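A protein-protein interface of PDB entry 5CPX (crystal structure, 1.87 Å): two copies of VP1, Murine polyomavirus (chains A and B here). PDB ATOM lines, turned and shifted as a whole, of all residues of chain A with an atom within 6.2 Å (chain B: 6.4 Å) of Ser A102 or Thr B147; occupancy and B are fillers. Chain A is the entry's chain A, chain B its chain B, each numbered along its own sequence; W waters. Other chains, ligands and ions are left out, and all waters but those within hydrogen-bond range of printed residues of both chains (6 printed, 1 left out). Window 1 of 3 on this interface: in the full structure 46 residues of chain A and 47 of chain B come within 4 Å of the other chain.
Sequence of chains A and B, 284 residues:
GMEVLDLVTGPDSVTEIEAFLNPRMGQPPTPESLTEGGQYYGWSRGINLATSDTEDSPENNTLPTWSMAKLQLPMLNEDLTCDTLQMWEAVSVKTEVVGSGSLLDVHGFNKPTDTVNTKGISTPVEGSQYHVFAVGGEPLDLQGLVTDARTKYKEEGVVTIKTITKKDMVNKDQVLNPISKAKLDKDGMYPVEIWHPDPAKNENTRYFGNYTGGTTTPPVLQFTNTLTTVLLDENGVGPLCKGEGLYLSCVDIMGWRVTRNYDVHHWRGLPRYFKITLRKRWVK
O of Gln A39 is in hydrogen-bond range of NE2 of Gln B174, 3.0 Å away.
O of Tyr A41 lies within hydrogen-bond range of NE2 of Gln B174, 2.8 Å away.
The backbone carbonyl oxygen (O) of Ser A102 is in hydrogen-bond range of the side-chain hydroxyl (OG1) of Thr B147 (2.7 Å).
The guanidinium group (NH2) of Arg A268 sits at hydrogen-bond distance from the backbone carbonyl oxygen (O) of Val B146 (3.2 Å).
The guanidinium group (NH1) of Arg A268 is in hydrogen-bond range of the backbone carbonyl oxygen (O) of Gln B174 (2.9 Å).
Water W1 lies within hydrogen-bond range of the side-chain hydroxyl (OH) of Tyr B130, a ring nitrogen (ND1) of His B196 and the backbone NH (N) of Gly A101.
Water W2 lies within hydrogen-bond range of OG of Ser A102 (2.7 Å), NH2 of Arg A268 (2.8 Å) and OG1 of Thr B147 (2.8 Å).
Water W3 lies within hydrogen-bond range of OE1 of Glu B193 (2.8 Å) and O of Leu A104 (3.2 Å).
Water W4 lies within hydrogen-bond range of O of Asp A105 (2.8 Å) and OG1 of Thr B147 (2.9 Å).
Water W5 lies within hydrogen-bond range of the side-chain carboxylate of Asp A105 (2.8 Å), the backbone NH of Asp B148 (2.9 Å), the side-chain hydroxyl of Thr B151 (3.0 Å) and the side-chain hydroxyl of Tyr B153 (3.4 Å).
Water W6 lies within hydrogen-bond range of O of Leu A104 (2.9 Å), N of Val A106 (2.9 Å) and OE1 of Glu B193 (3.5 Å).
Among the printed residues, merely in contact across the chains: Ser A102 with His B196 (3.3 Å), Asp A105 with Glu B193 (3.3 Å), Ser A102 with Glu B193 (3.4 Å), Gly A101 with Glu B193 (3.4 Å), Asp A105 with Thr B147 (3.4 Å), Trp A43 with Thr B147 (3.5 Å), Ser A102 with Leu B145 (3.5 Å), Arg A268 with Leu B145 (3.6 Å), Leu A104 with Tyr B130 (3.7 Å), Trp A43 with Gln B174 (3.7 Å), Gly A101 with Val B192 (3.7 Å), Gly A101 with His B196 (3.7 Å), Gly A99 with His B196 (3.8 Å), Gly A101 with Tyr B130 (3.8 Å), Leu A104 with Val B192 (3.8 Å) and Leu A104 with Glu B193 (3.9 Å).
The backbone NH (N) of Leu B145 is in hydrogen-bond range of the backbone carbonyl oxygen (O) of Ile B194 (2.8 Å).
The backbone carbonyl oxygen of Leu B145 is in hydrogen-bond range of a ring nitrogen (NE2) of His B196 (2.8 Å).
The backbone NH (N) of Val B146 is in hydrogen-bond range of the backbone carbonyl oxygen (O) of Asp B173.
The backbone NH (N) of Ala B149 sits at hydrogen-bond distance from the side-chain amide oxygen (OE1) of Gln B174 (2.8 Å).
The side-chain hydroxyl of Tyr B153 sits at hydrogen-bond distance from the side-chain carboxylate of Glu B193.
The backbone carbonyl oxygen (O) of Ile B194 is in hydrogen-bond range of a ring nitrogen (NE2) of His B196 (3.1 Å).
Hydrophobic or aromatic side chains of chain B that line the printed part of chain A: Tyr B130, Leu B145, Val B192 and His B196.
Along chain B the printed residues that touch a printed residue of chain A span positions 130 to 196.
Of the 15 printed residues of chain A, 9 touch a printed residue of chain B.
Hydrophobic or aromatic side chains of chain A within 4 Å of the printed part of chain B: Trp A43 and Leu A104.
Along chain A the printed residues that touch a printed residue of chain B span positions 39 to 268.
Among the printed residues, 21 pairs touch across the chains.
Among the printed residues, no Asp or Glu carboxylate lies within 4 Å of a Lys or Arg side-chain nitrogen of the other chain.
Ser A100 touches none of the printed residues of chain B.
Ser A102 touches four residues of chain B.
Printed residues of chain A within 4 Å of Tyr B130: Gly A101 (3.8 Å) and Leu A104 (3.7 Å).
Of the printed residues of chain A, Leu B145 touches Ser A102 and Arg A268.
Of the printed residues of chain A, Thr B147 touches Trp A43, Ser A102 and Asp A105.
The nearest residue of chain A that does not touch Thr B147 is Arg A268 (4.1 Å).
The nearest printed residue of chain B that does not touch Gly A99 is Leu B145 (4.2 Å).
No position is printed for both chains.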
ATOM      1  N   GLN A  39      -7.705   3.601  20.258  1.00  0.00           N
ATOM      2  CA  GLN A  39      -8.313   3.415  21.583  1.00  0.00           C
ATOM      3  C   GLN A  39      -9.643   4.176  21.769  1.00  0.00           C
ATOM      4  O   GLN A  39     -10.399   3.858  22.677  1.00  0.00           O
ATOM      5  CB  GLN A  39      -7.325   3.768  22.713  1.00  0.00           C
ATOM      6  CG  GLN A  39      -7.014   5.258  22.868  1.00  0.00           C
ATOM      7  CD  GLN A  39      -5.817   5.699  22.040  1.00  0.00           C
ATOM      8  OE1 GLN A  39      -5.646   5.272  20.893  1.00  0.00           O
ATOM      9  NE2 GLN A  39      -4.982   6.558  22.614  1.00  0.00           N
ATOM     10  N   TYR A  41     -11.976   4.248  19.271  1.00  0.00           N
ATOM     11  CA  TYR A  41     -12.967   3.660  18.358  1.00  0.00           C
ATOM     12  C   TYR A  41     -14.164   3.076  19.131  1.00  0.00           C
ATOM     13  O   TYR A  41     -13.992   2.321  20.096  1.00  0.00           O
ATOM     14  CB  TYR A  41     -12.305   2.633  17.415  1.00  0.00           C
ATOM     15  CG  TYR A  41     -13.217   2.063  16.341  1.00  0.00           C
ATOM     16  CD1 TYR A  41     -14.116   2.885  15.636  1.00  0.00           C
ATOM     17  CD2 TYR A  41     -13.143   0.716  15.985  1.00  0.00           C
ATOM     18  CE1 TYR A  41     -14.944   2.365  14.650  1.00  0.00           C
ATOM     19  CE2 TYR A  41     -13.952   0.187  14.986  1.00  0.00           C
ATOM     20  CZ  TYR A  41     -14.849   1.012  14.319  1.00  0.00           C
ATOM     21  OH  TYR A  41     -15.671   0.483  13.337  1.00  0.00           O
ATOM     22  N   TRP A  43     -16.208   5.418  20.279  1.00  0.00           N
ATOM     23  CA  TRP A  43     -16.396   6.635  21.075  1.00  0.00           C
ATOM     24  C   TRP A  43     -16.162   7.855  20.180  1.00  0.00           C
ATOM     25  O   TRP A  43     -15.594   7.736  19.100  1.00  0.00           O
ATOM     26  CB  TRP A  43     -15.374   6.722  22.232  1.00  0.00           C
ATOM     27  CG  TRP A  43     -15.309   5.500  23.104  1.00  0.00           C
ATOM     28  CD1 TRP A  43     -14.626   4.335  22.840  1.00  0.00           C
ATOM     29  CD2 TRP A  43     -15.936   5.316  24.383  1.00  0.00           C
ATOM     30  NE1 TRP A  43     -14.800   3.439  23.876  1.00  0.00           N
ATOM     31  CE2 TRP A  43     -15.596   4.012  24.834  1.00  0.00           C
ATOM     32  CE3 TRP A  43     -16.741   6.129  25.200  1.00  0.00           C
ATOM     33  CZ2 TRP A  43     -16.043   3.496  26.063  1.00  0.00           C
ATOM     34  CZ3 TRP A  43     -17.205   5.604  26.427  1.00  0.00           C
ATOM     35  CH2 TRP A  43     -16.846   4.303  26.840  1.00  0.00           C
ATOM     36  N   GLY A  99     -23.933  -5.252  23.434  1.00  0.00           N
ATOM     37  CA  GLY A  99     -22.804  -4.828  24.252  1.00  0.00           C
ATOM     38  C   GLY A  99     -23.118  -3.936  25.441  1.00  0.00           C
ATOM     39  O   GLY A  99     -22.204  -3.347  26.016  1.00  0.00           O
ATOM     40  N   SER A 100     -24.385  -3.843  25.847  1.00  0.00           N
ATOM     41  CA  SER A 100     -24.694  -2.987  27.005  1.00  0.00           C
ATOM     42  C   SER A 100     -23.975  -3.468  28.291  1.00  0.00           C
ATOM     43  O   SER A 100     -23.603  -2.663  29.141  1.00  0.00           O
ATOM     44  CB  SER A 100     -26.206  -2.841  27.223  1.00  0.00           C
ATOM     45  OG  SER A 100     -26.781  -4.088  27.542  1.00  0.00           O
ATOM     46  N   GLY A 101     -23.753  -4.780  28.406  1.00  0.00           N
ATOM     47  CA  GLY A 101     -22.963  -5.341  29.511  1.00  0.00           C
ATOM     48  C   GLY A 101     -21.561  -4.728  29.648  1.00  0.00           C
ATOM     49  O   GLY A 101     -21.013  -4.661  30.746  1.00  0.00           O
ATOM     50  N   SER A 102     -20.986  -4.253  28.550  1.00  0.00           N
ATOM     51  CA  SER A 102     -19.654  -3.627  28.593  1.00  0.00           C
ATOM     52  C   SER A 102     -19.666  -2.342  29.432  1.00  0.00           C
ATOM     53  O   SER A 102     -18.626  -1.911  29.938  1.00  0.00           O
ATOM     54  CB  SER A 102     -19.133  -3.324  27.185  1.00  0.00           C
ATOM     55  OG  SER A 102     -19.850  -2.236  26.583  1.00  0.00           O
ATOM     56  N   LEU A 103     -20.847  -1.742  29.591  1.00  0.00           N
ATOM     57  CA  LEU A 103     -20.979  -0.527  30.402  1.00  0.00           C
ATOM     58  C   LEU A 103     -20.844  -0.814  31.908  1.00  0.00           C
ATOM     59  O   LEU A 103     -20.786   0.111  32.720  1.00  0.00           O
ATOM     60  CB  LEU A 103     -22.295   0.204  30.087  1.00  0.00           C
ATOM     61  CG  LEU A 103     -22.528   0.570  28.603  1.00  0.00           C
ATOM     62  CD1 LEU A 103     -23.880   1.264  28.426  1.00  0.00           C
ATOM     63  CD2 LEU A 103     -21.403   1.435  28.063  1.00  0.00           C
ATOM     64  N   LEU A 104     -20.783  -2.096  32.263  1.00  0.00           N
ATOM     65  CA  LEU A 104     -20.549  -2.520  33.651  1.00  0.00           C
ATOM     66  C   LEU A 104     -19.064  -2.459  34.035  1.00  0.00           C
ATOM     67  O   LEU A 104     -18.702  -2.734  35.182  1.00  0.00           O
ATOM     68  CB  LEU A 104     -21.083  -3.938  33.883  1.00  0.00           C
ATOM     69  CG  LEU A 104     -22.590  -4.133  33.653  1.00  0.00           C
ATOM     70  CD1 LEU A 104     -22.900  -5.622  33.604  1.00  0.00           C
ATOM     71  CD2 LEU A 104     -23.410  -3.446  34.734  1.00  0.00           C
ATOM     72  N   ASP A 105     -18.211  -2.107  33.079  1.00  0.00           N
ATOM     73  CA  ASP A 105     -16.801  -1.816  33.392  1.00  0.00           C
ATOM     74  C   ASP A 105     -16.706  -0.484  34.162  1.00  0.00           C
ATOM     75  O   ASP A 105     -16.762   0.598  33.572  1.00  0.00           O
ATOM     76  CB  ASP A 105     -15.950  -1.784  32.105  1.00  0.00           C
ATOM     77  CG  ASP A 105     -14.517  -1.258  32.336  1.00  0.00           C
ATOM     78  OD1 ASP A 105     -14.174  -0.819  33.458  1.00  0.00           O
ATOM     79  OD2 ASP A 105     -13.728  -1.266  31.369  1.00  0.00           O
ATOM     80  N   VAL A 106     -16.578  -0.578  35.480  1.00  0.00           N
ATOM     81  CA  VAL A 106     -16.429   0.603  36.340  1.00  0.00           C
ATOM     82  C   VAL A 106     -15.072   0.570  37.050  1.00  0.00           C
ATOM     83  O   VAL A 106     -14.894   1.152  38.126  1.00  0.00           O
ATOM     84  CB  VAL A 106     -17.595   0.741  37.360  1.00  0.00           C
ATOM     85  CG1 VAL A 106     -18.915   0.969  36.616  1.00  0.00           C
ATOM     86  CG2 VAL A 106     -17.684  -0.477  38.283  1.00  0.00           C
ATOM     87  N   ASN A 110     -11.865   6.696  34.410  1.00  0.00           N
ATOM     88  CA  ASN A 110     -12.792   7.834  34.278  1.00  0.00           C
ATOM     89  C   ASN A 110     -12.800   8.658  35.562  1.00  0.00           C
ATOM     90  O   ASN A 110     -12.237   8.241  36.567  1.00  0.00           O
ATOM     91  CB  ASN A 110     -14.233   7.370  33.999  1.00  0.00           C
ATOM     92  CG  ASN A 110     -14.372   6.553  32.720  1.00  0.00           C
ATOM     93  OD1 ASN A 110     -13.507   6.583  31.845  1.00  0.00           O
ATOM     94  ND2 ASN A 110     -15.496   5.823  32.601  1.00  0.00           N
ATOM     95  N   ARG A 257     -18.829   9.022  28.610  1.00  0.00           N
ATOM     96  CA  ARG A 257     -17.927   8.894  29.757  1.00  0.00           C
ATOM     97  C   ARG A 257     -17.228  10.230  29.984  1.00  0.00           C
ATOM     98  O   ARG A 257     -17.126  11.058  29.066  1.00  0.00           O
ATOM     99  CB  ARG A 257     -16.895   7.777  29.573  1.00  0.00           C
ATOM    100  CG  ARG A 257     -15.848   8.052  28.509  1.00  0.00           C
ATOM    101  CD  ARG A 257     -14.789   6.955  28.519  1.00  0.00           C
ATOM    102  NE  ARG A 257     -13.676   7.317  27.661  1.00  0.00           N
ATOM    103  CZ  ARG A 257     -12.572   7.932  28.084  1.00  0.00           C
ATOM    104  NH1 ARG A 257     -12.406   8.232  29.370  1.00  0.00           N
ATOM    105  NH2 ARG A 257     -11.621   8.230  27.213  1.00  0.00           N
ATOM    106  N   ARG A 268     -20.424   7.633  23.746  1.00  0.00           N
ATOM    107  CA  ARG A 268     -20.327   6.177  23.546  1.00  0.00           C
ATOM    108  C   ARG A 268     -21.500   5.675  22.699  1.00  0.00           C
ATOM    109  O   ARG A 268     -22.667   5.992  22.979  1.00  0.00           O
ATOM    110  CB  ARG A 268     -20.305   5.422  24.893  1.00  0.00           C
ATOM    111  CG  ARG A 268     -20.257   3.877  24.802  1.00  0.00           C
ATOM    112  CD  ARG A 268     -19.065   3.362  23.993  1.00  0.00           C
ATOM    113  NE  ARG A 268     -18.662   1.994  24.331  1.00  0.00           N
ATOM    114  CZ  ARG A 268     -18.106   1.133  23.476  1.00  0.00           C
ATOM    115  NH1 ARG A 268     -17.948   1.461  22.191  1.00  0.00           N
ATOM    116  NH2 ARG A 268     -17.722  -0.066  23.904  1.00  0.00           N
ATOM    117  N   LEU A 270     -23.006   1.967  20.511  1.00  0.00           N
ATOM    118  CA  LEU A 270     -22.930   0.516  20.463  1.00  0.00           C
ATOM    119  C   LEU A 270     -23.395   0.013  19.097  1.00  0.00           C
ATOM    120  O   LEU A 270     -24.168   0.689  18.427  1.00  0.00           O
ATOM    121  CB  LEU A 270     -23.777  -0.111  21.589  1.00  0.00           C
ATOM    122  CG  LEU A 270     -23.217  -0.005  23.022  1.00  0.00           C
ATOM    123  CD1 LEU A 270     -24.208  -0.599  24.028  1.00  0.00           C
ATOM    124  CD2 LEU A 270     -21.852  -0.690  23.131  1.00  0.00           C
ATOM    125  N   TYR B 130     -28.205  -5.420  35.926  1.00  0.00           N
ATOM    126  CA  TYR B 130     -28.076  -6.184  34.695  1.00  0.00           C
ATOM    127  C   TYR B 130     -28.736  -7.534  34.928  1.00  0.00           C
ATOM    128  O   TYR B 130     -28.337  -8.265  35.828  1.00  0.00           O
ATOM    129  CB  TYR B 130     -26.592  -6.346  34.372  1.00  0.00           C
ATOM    130  CG  TYR B 130     -26.266  -6.921  33.000  1.00  0.00           C
ATOM    131  CD1 TYR B 130     -26.637  -6.255  31.821  1.00  0.00           C
ATOM    132  CD2 TYR B 130     -25.530  -8.104  32.891  1.00  0.00           C
ATOM    133  CE1 TYR B 130     -26.305  -6.772  30.563  1.00  0.00           C
ATOM    134  CE2 TYR B 130     -25.187  -8.620  31.650  1.00  0.00           C
ATOM    135  CZ  TYR B 130     -25.579  -7.960  30.491  1.00  0.00           C
ATOM    136  OH  TYR B 130     -25.217  -8.498  29.278  1.00  0.00           O
ATOM    137  N   LEU B 145     -17.285  -7.893  23.417  1.00  0.00           N
ATOM    138  CA  LEU B 145     -17.280  -6.440  23.181  1.00  0.00           C
ATOM    139  C   LEU B 145     -16.904  -5.770  24.495  1.00  0.00           C
ATOM    140  O   LEU B 145     -17.554  -6.010  25.512  1.00  0.00           O
ATOM    141  CB  LEU B 145     -18.646  -5.905  22.690  1.00  0.00           C
ATOM    142  CG  LEU B 145     -18.685  -4.435  22.231  1.00  0.00           C
ATOM    143  CD1 LEU B 145     -19.777  -4.235  21.175  1.00  0.00           C
ATOM    144  CD2 LEU B 145     -18.905  -3.445  23.373  1.00  0.00           C
ATOM    145  N   VAL B 146     -15.876  -4.924  24.470  1.00  0.00           N
ATOM    146  CA  VAL B 146     -15.374  -4.317  25.711  1.00  0.00           C
ATOM    147  C   VAL B 146     -15.398  -2.787  25.671  1.00  0.00           C
ATOM    148  O   VAL B 146     -15.403  -2.166  24.606  1.00  0.00           O
ATOM    149  CB  VAL B 146     -13.932  -4.798  26.071  1.00  0.00           C
ATOM    150  CG1 VAL B 146     -13.890  -6.315  26.255  1.00  0.00           C
ATOM    151  CG2 VAL B 146     -12.927  -4.373  25.007  1.00  0.00           C
ATOM    152  N   THR B 147     -15.369  -2.194  26.856  1.00  0.00           N
ATOM    153  CA  THR B 147     -15.187  -0.756  27.006  1.00  0.00           C
ATOM    154  C   THR B 147     -13.796  -0.322  26.498  1.00  0.00           C
ATOM    155  O   THR B 147     -13.671   0.682  25.775  1.00  0.00           O
ATOM    156  CB  THR B 147     -15.384  -0.349  28.487  1.00  0.00           C
ATOM    157  OG1 THR B 147     -16.793  -0.323  28.788  1.00  0.00           O
ATOM    158  CG2 THR B 147     -14.785   1.053  28.777  1.00  0.00           C
ATOM    159  N   ASP B 148     -12.765  -1.083  26.863  1.00  0.00           N
ATOM    160  CA  ASP B 148     -11.386  -0.689  26.577  1.00  0.00           C
ATOM    161  C   ASP B 148     -10.552  -1.893  26.166  1.00  0.00           C
ATOM    162  O   ASP B 148     -10.311  -2.791  26.982  1.00  0.00           O
ATOM    163  CB  ASP B 148     -10.779  -0.010  27.813  1.00  0.00           C
ATOM    164  CG  ASP B 148      -9.463   0.723  27.512  1.00  0.00           C
ATOM    165  OD1 ASP B 148      -8.853   0.492  26.453  1.00  0.00           O
ATOM    166  OD2 ASP B 148      -9.043   1.547  28.347  1.00  0.00           O
ATOM    167  N   ALA B 149     -10.115  -1.908  24.905  1.00  0.00           N
ATOM    168  CA  ALA B 149      -9.333  -3.022  24.366  1.00  0.00           C
ATOM    169  C   ALA B 149      -7.936  -3.088  24.991  1.00  0.00           C
ATOM    170  O   ALA B 149      -7.186  -4.038  24.741  1.00  0.00           O
ATOM    171  CB  ALA B 149      -9.215  -2.909  22.848  1.00  0.00           C
ATOM    172  N   THR B 151      -7.514  -2.983  28.321  1.00  0.00           N
ATOM    173  CA  THR B 151      -7.666  -3.561  29.669  1.00  0.00           C
ATOM    174  C   THR B 151      -6.835  -4.844  29.773  1.00  0.00           C
ATOM    175  O   THR B 151      -6.877  -5.692  28.879  1.00  0.00           O
ATOM    176  CB  THR B 151      -9.133  -3.884  29.998  1.00  0.00           C
ATOM    177  OG1 THR B 151      -9.914  -2.679  29.943  1.00  0.00           O
ATOM    178  CG2 THR B 151      -9.253  -4.503  31.397  1.00  0.00           C
ATOM    179  N   TYR B 153      -6.744  -7.915  31.437  1.00  0.00           N
ATOM    180  CA  TYR B 153      -7.362  -8.997  32.209  1.00  0.00           C
ATOM    181  C   TYR B 153      -6.322 -10.055  32.543  1.00  0.00           C
ATOM    182  O   TYR B 153      -5.360 -10.246  31.788  1.00  0.00           O
ATOM    183  CB  TYR B 153      -8.525  -9.635  31.441  1.00  0.00           C
ATOM    184  CG  TYR B 153      -9.663  -8.676  31.161  1.00  0.00           C
ATOM    185  CD1 TYR B 153     -10.557  -8.303  32.168  1.00  0.00           C
ATOM    186  CD2 TYR B 153      -9.842  -8.135  29.886  1.00  0.00           C
ATOM    187  CE1 TYR B 153     -11.598  -7.416  31.914  1.00  0.00           C
ATOM    188  CE2 TYR B 153     -10.878  -7.250  29.623  1.00  0.00           C
ATOM    189  CZ  TYR B 153     -11.748  -6.893  30.635  1.00  0.00           C
ATOM    190  OH  TYR B 153     -12.772  -6.012  30.351  1.00  0.00           O
ATOM    191  N   ASP B 173     -12.461  -4.541  18.950  1.00  0.00           N
ATOM    192  CA  ASP B 173     -13.114  -5.189  20.096  1.00  0.00           C
ATOM    193  C   ASP B 173     -13.936  -4.237  20.967  1.00  0.00           C
ATOM    194  O   ASP B 173     -14.700  -4.682  21.831  1.00  0.00           O
ATOM    195  CB  ASP B 173     -12.100  -6.005  20.924  1.00  0.00           C
ATOM    196  CG  ASP B 173     -11.542  -7.201  20.142  1.00  0.00           C
ATOM    197  OD1 ASP B 173     -12.303  -7.817  19.358  1.00  0.00           O
ATOM    198  OD2 ASP B 173     -10.341  -7.527  20.300  1.00  0.00           O
ATOM    199  N   GLN B 174     -13.793  -2.931  20.731  1.00  0.00           N
ATOM    200  CA  GLN B 174     -14.633  -1.928  21.403  1.00  0.00           C
ATOM    201  C   GLN B 174     -15.952  -1.704  20.669  1.00  0.00           C
ATOM    202  O   GLN B 174     -16.839  -1.017  21.174  1.00  0.00           O
ATOM    203  CB  GLN B 174     -13.866  -0.609  21.588  1.00  0.00           C
ATOM    204  CG  GLN B 174     -12.691  -0.803  22.538  1.00  0.00           C
ATOM    205  CD  GLN B 174     -11.804   0.414  22.733  1.00  0.00           C
ATOM    206  OE1 GLN B 174     -10.788   0.320  23.419  1.00  0.00           O
ATOM    207  NE2 GLN B 174     -12.173   1.554  22.142  1.00  0.00           N
ATOM    208  N   VAL B 192     -19.130 -10.671  32.452  1.00  0.00           N
ATOM    209  CA  VAL B 192     -20.265 -10.084  31.751  1.00  0.00           C
ATOM    210  C   VAL B 192     -19.922  -8.725  31.120  1.00  0.00           C
ATOM    211  O   VAL B 192     -20.610  -8.284  30.205  1.00  0.00           O
ATOM    212  CB  VAL B 192     -21.548 -10.011  32.616  1.00  0.00           C
ATOM    213  CG1 VAL B 192     -21.939 -11.414  33.082  1.00  0.00           C
ATOM    214  CG2 VAL B 192     -21.362  -9.079  33.807  1.00  0.00           C
ATOM    215  N   GLU B 193     -18.843  -8.083  31.568  1.00  0.00           N
ATOM    216  CA  GLU B 193     -18.410  -6.845  30.912  1.00  0.00           C
ATOM    217  C   GLU B 193     -17.712  -7.099  29.558  1.00  0.00           C
ATOM    218  O   GLU B 193     -17.431  -6.156  28.817  1.00  0.00           O
ATOM    219  CB  GLU B 193     -17.533  -5.995  31.835  1.00  0.00           C
ATOM    220  CG  GLU B 193     -16.115  -6.510  32.048  1.00  0.00           C
ATOM    221  CD  GLU B 193     -15.255  -5.483  32.777  1.00  0.00           C
ATOM    222  OE1 GLU B 193     -15.725  -4.923  33.792  1.00  0.00           O
ATOM    223  OE2 GLU B 193     -14.117  -5.218  32.330  1.00  0.00           O
ATOM    224  N   ILE B 194     -17.449  -8.371  29.254  1.00  0.00           N
ATOM    225  CA  ILE B 194     -16.771  -8.778  28.009  1.00  0.00           C
ATOM    226  C   ILE B 194     -17.716  -9.536  27.069  1.00  0.00           C
ATOM    227  O   ILE B 194     -17.730  -9.281  25.866  1.00  0.00           O
ATOM    228  CB  ILE B 194     -15.549  -9.684  28.286  1.00  0.00           C
ATOM    229  CG1 ILE B 194     -14.482  -8.948  29.114  1.00  0.00           C
ATOM    230  CG2 ILE B 194     -14.917 -10.167  26.970  1.00  0.00           C
ATOM    231  CD1 ILE B 194     -13.377  -9.873  29.621  1.00  0.00           C
ATOM    232  N   HIS B 196     -21.296 -11.077  25.616  1.00  0.00           N
ATOM    233  CA  HIS B 196     -22.704 -10.728  25.414  1.00  0.00           C
ATOM    234  C   HIS B 196     -23.374 -11.799  24.573  1.00  0.00           C
ATOM    235  O   HIS B 196     -22.696 -12.469  23.788  1.00  0.00           O
ATOM    236  CB  HIS B 196     -22.758  -9.376  24.689  1.00  0.00           C
ATOM    237  CG  HIS B 196     -21.790  -8.400  25.272  1.00  0.00           C
ATOM    238  ND1 HIS B 196     -22.024  -7.759  26.470  1.00  0.00           N
ATOM    239  CD2 HIS B 196     -20.544  -8.037  24.884  1.00  0.00           C
ATOM    240  CE1 HIS B 196     -20.974  -7.013  26.777  1.00  0.00           C
ATOM    241  NE2 HIS B 196     -20.062  -7.168  25.832  1.00  0.00           N
HETATM  242  O   HOH W   1     -24.722  -7.164  26.953  1.00  0.00           O
HETATM  243  O   HOH W   2     -18.553   0.172  26.611  1.00  0.00           O
HETATM  244  O   HOH W   3     -17.706  -5.789  35.510  1.00  0.00           O
HETATM  245  O   HOH W   4     -17.368   1.503  30.988  1.00  0.00           O
HETATM  246  O   HOH W   5     -12.808  -2.854  29.201  1.00  0.00           O
HETATM  247  O   HOH W   6     -16.335  -3.203  36.753  1.00  0.00           O
